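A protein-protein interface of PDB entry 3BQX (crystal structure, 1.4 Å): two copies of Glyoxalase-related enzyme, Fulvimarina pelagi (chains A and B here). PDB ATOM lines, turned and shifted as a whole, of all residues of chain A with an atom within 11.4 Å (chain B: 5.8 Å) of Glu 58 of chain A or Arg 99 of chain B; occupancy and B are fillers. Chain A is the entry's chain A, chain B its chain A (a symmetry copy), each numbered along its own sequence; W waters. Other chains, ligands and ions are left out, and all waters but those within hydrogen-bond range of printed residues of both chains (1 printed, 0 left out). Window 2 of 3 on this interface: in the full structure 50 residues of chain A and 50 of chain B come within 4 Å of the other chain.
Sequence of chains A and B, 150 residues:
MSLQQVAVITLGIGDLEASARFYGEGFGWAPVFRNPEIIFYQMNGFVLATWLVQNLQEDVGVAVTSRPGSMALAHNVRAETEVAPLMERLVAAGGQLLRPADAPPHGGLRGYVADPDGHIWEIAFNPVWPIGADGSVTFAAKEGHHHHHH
O of Leu 98 of chain B touches O of Val 60 of chain A (3.9 Å).
O of Val 60 of chain A touches CB of Arg 99 of chain B, 3.4 Å away.
Tyr 112 of chain B touches Val 60 of chain A (CE2 to CA, 3.6 Å).
Gly 61 of chain A touches Arg 99 of chain B.
The side-chain carboxylate of Asp 102 of chain B lies within salt-bridge range of the guanidinium group of Arg 110 of chain B (2.6 Å).
The backbone carbonyl oxygen (O) of Arg 99 of chain B sits at hydrogen-bond distance from the backbone NH (N) of Tyr 112 of chain B (2.9 Å).
NE of Arg 99 of chain B is in salt-bridge range of OD2 of Asp 102 of chain B (2.9 Å).
The backbone NH of Leu 98 of chain B sits at hydrogen-bond distance from the backbone carbonyl oxygen of Tyr 112 of chain B, 3.0 Å away.
Printed residues of chain A within 4 Å of Arg 99 of chain B: Glu 58 (3.5 Å), Asp 59 (2.8 Å), Val 60 (3.4 Å) and Gly 61 (3.99 Å).
No residue of chain A comes within 4 Å of Leu 97 of chain B.
Pro 100 of chain B touches none of the printed residues of chain A.
No residue of chain A comes within 4 Å of Ala 101 of chain B.
No residue of chain A comes within 4 Å of Gly 111 of chain B.
Tyr 112 of chain B touches just these residues of chain A: Asp 59 (2.5 Å) and Val 60 (3.6 Å).
Printed residues of chain B within 4 Å of Gly 61 of chain A: Arg 99 (3.99 Å).
Printed residues of chain B within 4 Å of Val 60 of chain A: Leu 98, Arg 99 and Tyr 112.
Of the printed residues of chain B, Asp 59 of chain A touches Arg 99 (2.8 Å), Arg 110 (2.9 Å) and Tyr 112 (2.5 Å).
Leu 56 of chain A touches none of the printed residues of chain B.
The nearest printed residue of chain A that does not touch Arg 99 of chain B is Val 62 of chain A (6.0 Å).
The nearest printed residue of chain B that does not touch Val 60 of chain A is Arg 110 of chain B (5.9 Å).
O of Asp 59 of chain A is in hydrogen-bond range of NH1 of Arg 99 of chain B, 2.8 Å away.
O of Glu 58 of chain A lies within hydrogen-bond range of NH1 of Arg 99 of chain B (3.5 Å).
OD1 of Asp 59 of chain A lies within salt-bridge range of NH2 of Arg 110 of chain B (2.9 Å).
The side-chain carboxylate of Asp 59 of chain A lies within hydrogen-bond range of the side-chain hydroxyl of Tyr 112 of chain B (2.5 Å).
Water W1 bridges the backbone carbonyl oxygen (O) of Leu 98 of chain B (2.7 Å) and the backbone carbonyl oxygen (O) of Val 60 of chain A (2.9 Å).
No position is printed for both chains.
Of the 11 printed residues of chain B, 4 touch a printed residue of chain A.
Hydrophobic or aromatic side chains of chain A within 4 Å of the printed part of chain B: Val 60.
Among the printed residues, 8 pairs touch across the chains.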
ATOM      1  N   THR A  10     -19.047 -28.231 -16.238  1.00  0.00           N
ATOM      2  CA  THR A  10     -18.316 -29.401 -15.776  1.00  0.00           C
ATOM      3  C   THR A  10     -19.241 -30.346 -15.044  1.00  0.00           C
ATOM      4  O   THR A  10     -19.911 -29.960 -14.089  1.00  0.00           O
ATOM      5  CB  THR A  10     -17.172 -29.013 -14.827  1.00  0.00           C
ATOM      6  OG1 THR A  10     -16.227 -28.203 -15.532  1.00  0.00           O
ATOM      7  CG2 THR A  10     -16.452 -30.249 -14.306  1.00  0.00           C
ATOM      8  N   GLY A  12     -19.515 -33.884 -12.904  1.00  0.00           N
ATOM      9  CA  GLY A  12     -18.719 -34.836 -12.148  1.00  0.00           C
ATOM     10  C   GLY A  12     -19.169 -36.231 -12.539  1.00  0.00           C
ATOM     11  O   GLY A  12     -20.367 -36.515 -12.557  1.00  0.00           O
ATOM     12  N   ILE A  13     -18.217 -37.107 -12.854  1.00  0.00           N
ATOM     13  CA  ILE A  13     -18.535 -38.470 -13.271  1.00  0.00           C
ATOM     14  C   ILE A  13     -17.746 -39.519 -12.493  1.00  0.00           C
ATOM     15  O   ILE A  13     -16.766 -39.203 -11.830  1.00  0.00           O
ATOM     16  CB  ILE A  13     -18.263 -38.648 -14.779  1.00  0.00           C
ATOM     17  CG1 ILE A  13     -16.778 -38.412 -15.069  1.00  0.00           C
ATOM     18  CG2 ILE A  13     -19.130 -37.666 -15.581  1.00  0.00           C
ATOM     19  CD1 ILE A  13     -16.333 -38.898 -16.440  1.00  0.00           C
ATOM     20  N   ASN A  35      -7.636 -37.164 -20.845  1.00  0.00           N
ATOM     21  CA  ASN A  35      -6.565 -37.766 -20.068  1.00  0.00           C
ATOM     22  C   ASN A  35      -7.275 -38.685 -19.071  1.00  0.00           C
ATOM     23  O   ASN A  35      -8.503 -38.740 -19.051  1.00  0.00           O
ATOM     24  CB  ASN A  35      -5.658 -36.717 -19.394  1.00  0.00           C
ATOM     25  CG  ASN A  35      -6.348 -35.931 -18.304  1.00  0.00           C
ATOM     26  OD1 ASN A  35      -7.333 -36.371 -17.726  1.00  0.00           O
ATOM     27  ND2 ASN A  35      -5.801 -34.760 -17.997  1.00  0.00           N
ATOM     28  N   GLU A  37      -8.285 -38.460 -16.163  1.00  0.00           N
ATOM     29  CA  GLU A  37      -9.251 -37.900 -15.222  1.00  0.00           C
ATOM     30  C   GLU A  37     -10.293 -36.944 -15.791  1.00  0.00           C
ATOM     31  O   GLU A  37     -11.288 -36.660 -15.126  1.00  0.00           O
ATOM     32  CB  GLU A  37      -8.524 -37.204 -14.063  1.00  0.00           C
ATOM     33  CG  GLU A  37      -7.852 -35.894 -14.426  1.00  0.00           C
ATOM     34  CD  GLU A  37      -7.165 -35.242 -13.237  1.00  0.00           C
ATOM     35  OE1 GLU A  37      -6.194 -35.836 -12.721  1.00  0.00           O
ATOM     36  OE2 GLU A  37      -7.597 -34.143 -12.816  1.00  0.00           O
ATOM     37  N   ILE A  38     -10.091 -36.451 -17.006  1.00  0.00           N
ATOM     38  CA  ILE A  38     -11.047 -35.501 -17.563  1.00  0.00           C
ATOM     39  C   ILE A  38     -11.152 -35.568 -19.081  1.00  0.00           C
ATOM     40  O   ILE A  38     -10.205 -35.961 -19.767  1.00  0.00           O
ATOM     41  CB  ILE A  38     -10.650 -34.055 -17.144  1.00  0.00           C
ATOM     42  CG1 ILE A  38     -11.812 -33.082 -17.344  1.00  0.00           C
ATOM     43  CG2 ILE A  38      -9.437 -33.596 -17.937  1.00  0.00           C
ATOM     44  CD1 ILE A  38     -11.583 -31.720 -16.654  1.00  0.00           C
ATOM     45  N   TRP A  51     -15.404 -34.608 -15.584  1.00  0.00           N
ATOM     46  CA  TRP A  51     -14.273 -34.781 -14.679  1.00  0.00           C
ATOM     47  C   TRP A  51     -14.601 -35.781 -13.575  1.00  0.00           C
ATOM     48  O   TRP A  51     -15.695 -35.739 -13.022  1.00  0.00           O
ATOM     49  CB  TRP A  51     -13.997 -33.410 -14.058  1.00  0.00           C
ATOM     50  CG  TRP A  51     -12.648 -33.162 -13.504  1.00  0.00           C
ATOM     51  CD1 TRP A  51     -11.542 -33.958 -13.612  1.00  0.00           C
ATOM     52  CD2 TRP A  51     -12.224 -31.972 -12.830  1.00  0.00           C
ATOM     53  NE1 TRP A  51     -10.453 -33.327 -13.053  1.00  0.00           N
ATOM     54  CE2 TRP A  51     -10.845 -32.108 -12.567  1.00  0.00           C
ATOM     55  CE3 TRP A  51     -12.879 -30.799 -12.428  1.00  0.00           C
ATOM     56  CZ2 TRP A  51     -10.105 -31.116 -11.919  1.00  0.00           C
ATOM     57  CZ3 TRP A  51     -12.140 -29.810 -11.785  1.00  0.00           C
ATOM     58  CH2 TRP A  51     -10.767 -29.976 -11.540  1.00  0.00           C
ATOM     59  N   LEU A  52     -13.667 -36.676 -13.250  1.00  0.00           N
ATOM     60  CA  LEU A  52     -13.918 -37.630 -12.171  1.00  0.00           C
ATOM     61  C   LEU A  52     -14.298 -36.822 -10.932  1.00  0.00           C
ATOM     62  O   LEU A  52     -13.625 -35.852 -10.592  1.00  0.00           O
ATOM     63  CB  LEU A  52     -12.669 -38.468 -11.882  1.00  0.00           C
ATOM     64  CG  LEU A  52     -12.303 -39.482 -12.966  1.00  0.00           C
ATOM     65  CD1 LEU A  52     -11.021 -40.202 -12.581  1.00  0.00           C
ATOM     66  CD2 LEU A  52     -13.444 -40.475 -13.143  1.00  0.00           C
ATOM     67  N   VAL A  53     -15.371 -37.234 -10.262  1.00  0.00           N
ATOM     68  CA  VAL A  53     -15.868 -36.524  -9.085  1.00  0.00           C
ATOM     69  C   VAL A  53     -14.827 -36.228  -8.011  1.00  0.00           C
ATOM     70  O   VAL A  53     -14.814 -35.134  -7.452  1.00  0.00           O
ATOM     71  CB  VAL A  53     -17.035 -37.285  -8.426  1.00  0.00           C
ATOM     72  CG1 VAL A  53     -17.675 -36.420  -7.347  1.00  0.00           C
ATOM     73  CG2 VAL A  53     -18.059 -37.672  -9.468  1.00  0.00           C
ATOM     74  N   GLN A  54     -13.952 -37.187  -7.714  1.00  0.00           N
ATOM     75  CA  GLN A  54     -12.936 -36.970  -6.688  1.00  0.00           C
ATOM     76  C   GLN A  54     -12.104 -35.732  -7.005  1.00  0.00           C
ATOM     77  O   GLN A  54     -11.793 -34.934  -6.122  1.00  0.00           O
ATOM     78  CB  GLN A  54     -11.983 -38.169  -6.572  1.00  0.00           C
ATOM     79  CG  GLN A  54     -12.618 -39.545  -6.595  1.00  0.00           C
ATOM     80  CD  GLN A  54     -12.717 -40.111  -8.002  1.00  0.00           C
ATOM     81  OE1 GLN A  54     -13.645 -39.799  -8.744  1.00  0.00           O
ATOM     82  NE2 GLN A  54     -11.743 -40.939  -8.379  1.00  0.00           N
ATOM     83  N   ASN A  55     -11.738 -35.588  -8.276  1.00  0.00           N
ATOM     84  CA  ASN A  55     -10.929 -34.466  -8.728  1.00  0.00           C
ATOM     85  C   ASN A  55     -11.700 -33.150  -8.683  1.00  0.00           C
ATOM     86  O   ASN A  55     -11.148 -32.112  -8.310  1.00  0.00           O
ATOM     87  CB  ASN A  55     -10.417 -34.742 -10.145  1.00  0.00           C
ATOM     88  CG  ASN A  55      -9.437 -35.903 -10.190  1.00  0.00           C
ATOM     89  OD1 ASN A  55      -8.296 -35.783  -9.744  1.00  0.00           O
ATOM     90  ND2 ASN A  55      -9.884 -37.036 -10.715  1.00  0.00           N
ATOM     91  N   LEU A  56     -12.973 -33.188  -9.061  1.00  0.00           N
ATOM     92  CA  LEU A  56     -13.786 -31.978  -9.017  1.00  0.00           C
ATOM     93  C   LEU A  56     -13.908 -31.515  -7.568  1.00  0.00           C
ATOM     94  O   LEU A  56     -13.706 -30.343  -7.259  1.00  0.00           O
ATOM     95  CB  LEU A  56     -15.178 -32.248  -9.593  1.00  0.00           C
ATOM     96  CG  LEU A  56     -16.232 -31.155  -9.382  1.00  0.00           C
ATOM     97  CD1 LEU A  56     -15.772 -29.826  -9.986  1.00  0.00           C
ATOM     98  CD2 LEU A  56     -17.531 -31.610 -10.019  1.00  0.00           C
ATOM     99  N   GLN A  57     -14.226 -32.456  -6.681  1.00  0.00           N
ATOM    100  CA  GLN A  57     -14.383 -32.158  -5.262  1.00  0.00           C
ATOM    101  C   GLN A  57     -13.099 -31.571  -4.689  1.00  0.00           C
ATOM    102  O   GLN A  57     -13.132 -30.642  -3.875  1.00  0.00           O
ATOM    103  CB  GLN A  57     -14.751 -33.436  -4.507  1.00  0.00           C
ATOM    104  CG  GLN A  57     -15.014 -33.238  -3.028  1.00  0.00           C
ATOM    105  CD  GLN A  57     -15.411 -34.526  -2.341  1.00  0.00           C
ATOM    106  OE1 GLN A  57     -14.602 -35.445  -2.203  1.00  0.00           O
ATOM    107  NE2 GLN A  57     -16.666 -34.607  -1.915  1.00  0.00           N
ATOM    108  N   GLU A  58     -11.969 -32.122  -5.119  1.00  0.00           N
ATOM    109  CA  GLU A  58     -10.658 -31.667  -4.668  1.00  0.00           C
ATOM    110  C   GLU A  58     -10.401 -30.220  -5.081  1.00  0.00           C
ATOM    111  O   GLU A  58      -9.856 -29.429  -4.308  1.00  0.00           O
ATOM    112  CB  GLU A  58      -9.569 -32.563  -5.263  1.00  0.00           C
ATOM    113  CG  GLU A  58      -8.147 -32.115  -4.962  1.00  0.00           C
ATOM    114  CD  GLU A  58      -7.109 -32.847  -5.802  1.00  0.00           C
ATOM    115  OE1 GLU A  58      -5.898 -32.635  -5.572  1.00  0.00           O
ATOM    116  OE2 GLU A  58      -7.501 -33.633  -6.696  1.00  0.00           O
ATOM    117  N   ASP A  59     -10.798 -29.877  -6.304  1.00  0.00           N
ATOM    118  CA  ASP A  59     -10.585 -28.529  -6.813  1.00  0.00           C
ATOM    119  C   ASP A  59     -11.448 -27.496  -6.093  1.00  0.00           C
ATOM    120  O   ASP A  59     -10.983 -26.400  -5.794  1.00  0.00           O
ATOM    121  CB  ASP A  59     -10.859 -28.481  -8.317  1.00  0.00           C
ATOM    122  CG  ASP A  59     -10.164 -27.317  -8.993  1.00  0.00           C
ATOM    123  OD1 ASP A  59      -8.915 -27.272  -8.952  1.00  0.00           O
ATOM    124  OD2 ASP A  59     -10.857 -26.449  -9.558  1.00  0.00           O
ATOM    125  N   VAL A  60     -12.701 -27.841  -5.817  1.00  0.00           N
ATOM    126  CA  VAL A  60     -13.594 -26.920  -5.116  1.00  0.00           C
ATOM    127  C   VAL A  60     -13.142 -26.733  -3.667  1.00  0.00           C
ATOM    128  O   VAL A  60     -13.321 -25.664  -3.084  1.00  0.00           O
ATOM    129  CB  VAL A  60     -15.054 -27.427  -5.141  1.00  0.00           C
ATOM    130  CG1 VAL A  60     -15.948 -26.499  -4.322  1.00  0.00           C
ATOM    131  CG2 VAL A  60     -15.547 -27.498  -6.581  1.00  0.00           C
ATOM    132  N   GLY A  61     -12.556 -27.773  -3.084  1.00  0.00           N
ATOM    133  CA  GLY A  61     -12.084 -27.665  -1.715  1.00  0.00           C
ATOM    134  C   GLY A  61     -13.079 -28.127  -0.668  1.00  0.00           C
ATOM    135  O   GLY A  61     -12.711 -28.357   0.483  1.00  0.00           O
ATOM    136  N   VAL A  62     -14.345 -28.248  -1.052  1.00  0.00           N
ATOM    137  CA  VAL A  62     -15.366 -28.707  -0.122  1.00  0.00           C
ATOM    138  C   VAL A  62     -16.004 -29.971  -0.673  1.00  0.00           C
ATOM    139  O   VAL A  62     -15.882 -30.275  -1.864  1.00  0.00           O
ATOM    140  CB  VAL A  62     -16.466 -27.638   0.106  1.00  0.00           C
ATOM    141  CG1 VAL A  62     -15.848 -26.368   0.666  1.00  0.00           C
ATOM    142  CG2 VAL A  62     -17.203 -27.351  -1.191  1.00  0.00           C
ATOM    143  N   ALA A  63     -16.671 -30.718   0.197  1.00  0.00           N
ATOM    144  CA  ALA A  63     -17.325 -31.945  -0.220  1.00  0.00           C
ATOM    145  C   ALA A  63     -18.361 -31.628  -1.284  1.00  0.00           C
ATOM    146  O   ALA A  63     -19.237 -30.781  -1.086  1.00  0.00           O
ATOM    147  CB  ALA A  63     -17.989 -32.630   0.974  1.00  0.00           C
ATOM    148  N   VAL A  64     -18.235 -32.299  -2.422  1.00  0.00           N
ATOM    149  CA  VAL A  64     -19.154 -32.133  -3.535  1.00  0.00           C
ATOM    150  C   VAL A  64     -19.750 -33.505  -3.813  1.00  0.00           C
ATOM    151  O   VAL A  64     -19.026 -34.461  -4.099  1.00  0.00           O
ATOM    152  CB  VAL A  64     -18.429 -31.624  -4.799  1.00  0.00           C
ATOM    153  CG1 VAL A  64     -19.413 -31.512  -5.953  1.00  0.00           C
ATOM    154  CG2 VAL A  64     -17.787 -30.278  -4.521  1.00  0.00           C
ATOM    155  N   THR A  65     -21.071 -33.599  -3.718  1.00  0.00           N
ATOM    156  CA  THR A  65     -21.770 -34.856  -3.941  1.00  0.00           C
ATOM    157  C   THR A  65     -21.477 -35.475  -5.305  1.00  0.00           C
ATOM    158  O   THR A  65     -21.147 -34.773  -6.261  1.00  0.00           O
ATOM    159  CB  THR A  65     -23.287 -34.668  -3.808  1.00  0.00           C
ATOM    160  OG1 THR A  65     -23.939 -35.929  -3.988  1.00  0.00           O
ATOM    161  CG2 THR A  65     -23.791 -33.684  -4.851  1.00  0.00           C
ATOM    162  N   SER A  66     -21.599 -36.797  -5.385  1.00  0.00           N
ATOM    163  CA  SER A  66     -21.359 -37.517  -6.629  1.00  0.00           C
ATOM    164  C   SER A  66     -22.678 -37.717  -7.365  1.00  0.00           C
ATOM    165  O   SER A  66     -22.702 -38.138  -8.523  1.00  0.00           O
ATOM    166  CB  SER A  66     -20.729 -38.882  -6.340  1.00  0.00           C
ATOM    167  OG  SER A  66     -21.628 -39.708  -5.620  1.00  0.00           O
ATOM    168  N   MET B  87     -15.941 -12.091  -7.694  1.00  0.00           N
ATOM    169  CA  MET B  87     -16.333 -12.992  -6.621  1.00  0.00           C
ATOM    170  C   MET B  87     -16.920 -12.237  -5.430  1.00  0.00           C
ATOM    171  O   MET B  87     -17.878 -12.699  -4.815  1.00  0.00           O
ATOM    172  CB  MET B  87     -15.139 -13.833  -6.172  1.00  0.00           C
ATOM    173  CG  MET B  87     -14.816 -14.964  -7.133  1.00  0.00           C
ATOM    174  SD  MET B  87     -13.248 -15.957  -6.621  1.00  0.00           S
ATOM    175  CE  MET B  87     -13.835 -16.640  -4.907  1.00  0.00           C
ATOM    176  N   LEU B  97     -19.274 -18.194  -0.558  1.00  0.00           N
ATOM    177  CA  LEU B  97     -17.873 -18.389  -0.898  1.00  0.00           C
ATOM    178  C   LEU B  97     -17.450 -19.811  -0.537  1.00  0.00           C
ATOM    179  O   LEU B  97     -17.566 -20.229   0.616  1.00  0.00           O
ATOM    180  CB  LEU B  97     -17.009 -17.374  -0.140  1.00  0.00           C
ATOM    181  CG  LEU B  97     -15.494 -17.416  -0.352  1.00  0.00           C
ATOM    182  CD1 LEU B  97     -15.153 -17.252  -1.826  1.00  0.00           C
ATOM    183  CD2 LEU B  97     -14.851 -16.306   0.469  1.00  0.00           C
ATOM    184  N   LEU B  98     -16.966 -20.552  -1.529  1.00  0.00           N
ATOM    185  CA  LEU B  98     -16.526 -21.929  -1.316  1.00  0.00           C
ATOM    186  C   LEU B  98     -15.009 -22.039  -1.337  1.00  0.00           C
ATOM    187  O   LEU B  98     -14.424 -22.816  -0.584  1.00  0.00           O
ATOM    188  CB  LEU B  98     -17.129 -22.857  -2.383  1.00  0.00           C
ATOM    189  CG  LEU B  98     -18.649 -23.035  -2.367  1.00  0.00           C
ATOM    190  CD1 LEU B  98     -19.069 -23.925  -3.535  1.00  0.00           C
ATOM    191  CD2 LEU B  98     -19.091 -23.641  -1.042  1.00  0.00           C
ATOM    192  N   ARG B  99     -14.371 -21.259  -2.201  1.00  0.00           N
ATOM    193  CA  ARG B  99     -12.921 -21.280  -2.291  1.00  0.00           C
ATOM    194  C   ARG B  99     -12.360 -19.948  -2.770  1.00  0.00           C
ATOM    195  O   ARG B  99     -12.630 -19.519  -3.889  1.00  0.00           O
ATOM    196  CB  ARG B  99     -12.457 -22.396  -3.237  1.00  0.00           C
ATOM    197  CG  ARG B  99     -10.951 -22.430  -3.421  1.00  0.00           C
ATOM    198  CD  ARG B  99     -10.481 -23.700  -4.108  1.00  0.00           C
ATOM    199  NE  ARG B  99      -9.026 -23.808  -4.038  1.00  0.00           N
ATOM    200  CZ  ARG B  99      -8.362 -24.954  -3.924  1.00  0.00           C
ATOM    201  NH1 ARG B  99      -9.017 -26.105  -3.870  1.00  0.00           N
ATOM    202  NH2 ARG B  99      -7.039 -24.945  -3.841  1.00  0.00           N
ATOM    203  N   PRO B 100     -11.596 -19.254  -1.911  1.00  0.00           N
ATOM    204  CA  PRO B 100     -11.014 -17.971  -2.308  1.00  0.00           C
ATOM    205  C   PRO B 100     -10.091 -18.210  -3.503  1.00  0.00           C
ATOM    206  O   PRO B 100      -9.471 -19.269  -3.615  1.00  0.00           O
ATOM    207  CB  PRO B 100     -10.251 -17.542  -1.059  1.00  0.00           C
ATOM    208  CG  PRO B 100     -11.079 -18.118   0.042  1.00  0.00           C
ATOM    209  CD  PRO B 100     -11.390 -19.504  -0.473  1.00  0.00           C
ATOM    210  N   ALA B 101      -9.996 -17.226  -4.386  1.00  0.00           N
ATOM    211  CA  ALA B 101      -9.167 -17.347  -5.576  1.00  0.00           C
ATOM    212  C   ALA B 101      -7.700 -17.659  -5.298  1.00  0.00           C
ATOM    213  O   ALA B 101      -7.052 -17.001  -4.484  1.00  0.00           O
ATOM    214  CB  ALA B 101      -9.270 -16.072  -6.405  1.00  0.00           C
ATOM    215  N   ASP B 102      -7.189 -18.677  -5.984  1.00  0.00           N
ATOM    216  CA  ASP B 102      -5.791 -19.073  -5.871  1.00  0.00           C
ATOM    217  C   ASP B 102      -5.390 -19.746  -7.178  1.00  0.00           C
ATOM    218  O   ASP B 102      -6.249 -20.058  -8.006  1.00  0.00           O
ATOM    219  CB  ASP B 102      -5.563 -20.018  -4.681  1.00  0.00           C
ATOM    220  CG  ASP B 102      -6.305 -21.332  -4.816  1.00  0.00           C
ATOM    221  OD1 ASP B 102      -6.122 -22.025  -5.837  1.00  0.00           O
ATOM    222  OD2 ASP B 102      -7.065 -21.679  -3.888  1.00  0.00           O
ATOM    223  N   ARG B 110      -8.262 -19.010 -10.023  1.00  0.00           N
ATOM    224  CA  ARG B 110      -9.680 -19.338  -9.964  1.00  0.00           C
ATOM    225  C   ARG B 110     -10.189 -19.579  -8.553  1.00  0.00           C
ATOM    226  O   ARG B 110      -9.453 -20.047  -7.677  1.00  0.00           O
ATOM    227  CB  ARG B 110      -9.985 -20.564 -10.841  1.00  0.00           C
ATOM    228  CG  ARG B 110      -9.361 -21.880 -10.373  1.00  0.00           C
ATOM    229  CD  ARG B 110     -10.228 -22.603  -9.345  1.00  0.00           C
ATOM    230  NE  ARG B 110      -9.552 -23.790  -8.822  1.00  0.00           N
ATOM    231  CZ  ARG B 110      -8.535 -23.753  -7.966  1.00  0.00           C
ATOM    232  NH1 ARG B 110      -8.076 -22.586  -7.526  1.00  0.00           N
ATOM    233  NH2 ARG B 110      -7.966 -24.880  -7.562  1.00  0.00           N
ATOM    234  N   GLY B 111     -11.456 -19.238  -8.345  1.00  0.00           N
ATOM    235  CA  GLY B 111     -12.109 -19.429  -7.065  1.00  0.00           C
ATOM    236  C   GLY B 111     -13.501 -19.988  -7.301  1.00  0.00           C
ATOM    237  O   GLY B 111     -13.923 -20.127  -8.452  1.00  0.00           O
ATOM    238  N   TYR B 112     -14.219 -20.310  -6.233  1.00  0.00           N
ATOM    239  CA  TYR B 112     -15.565 -20.860  -6.358  1.00  0.00           C
ATOM    240  C   TYR B 112     -16.572 -20.157  -5.460  1.00  0.00           C
ATOM    241  O   TYR B 112     -16.275 -19.830  -4.306  1.00  0.00           O
ATOM    242  CB  TYR B 112     -15.566 -22.353  -6.020  1.00  0.00           C
ATOM    243  CG  TYR B 112     -14.945 -23.256  -7.064  1.00  0.00           C
ATOM    244  CD1 TYR B 112     -15.690 -23.710  -8.156  1.00  0.00           C
ATOM    245  CD2 TYR B 112     -13.625 -23.705  -6.935  1.00  0.00           C
ATOM    246  CE1 TYR B 112     -15.142 -24.594  -9.082  1.00  0.00           C
ATOM    247  CE2 TYR B 112     -13.071 -24.584  -7.860  1.00  0.00           C
ATOM    248  CZ  TYR B 112     -13.837 -25.028  -8.928  1.00  0.00           C
ATOM    249  OH  TYR B 112     -13.317 -25.936  -9.823  1.00  0.00           O
ATOM    250  N   VAL B 113     -17.768 -19.927  -5.996  1.00  0.00           N
ATOM    251  CA  VAL B 113     -18.857 -19.297  -5.263  1.00  0.00           C
ATOM    252  C   VAL B 113     -20.137 -19.975  -5.715  1.00  0.00           C
ATOM    253  O   VAL B 113     -20.363 -20.129  -6.917  1.00  0.00           O
ATOM    254  CB  VAL B 113     -18.962 -17.783  -5.574  1.00  0.00           C
ATOM    255  CG1 VAL B 113     -20.168 -17.187  -4.861  1.00  0.00           C
ATOM    256  CG2 VAL B 113     -17.689 -17.067  -5.147  1.00  0.00           C
HETATM  257  O   HOH W   1     -12.409 -24.576  -0.584  1.00  0.00           O
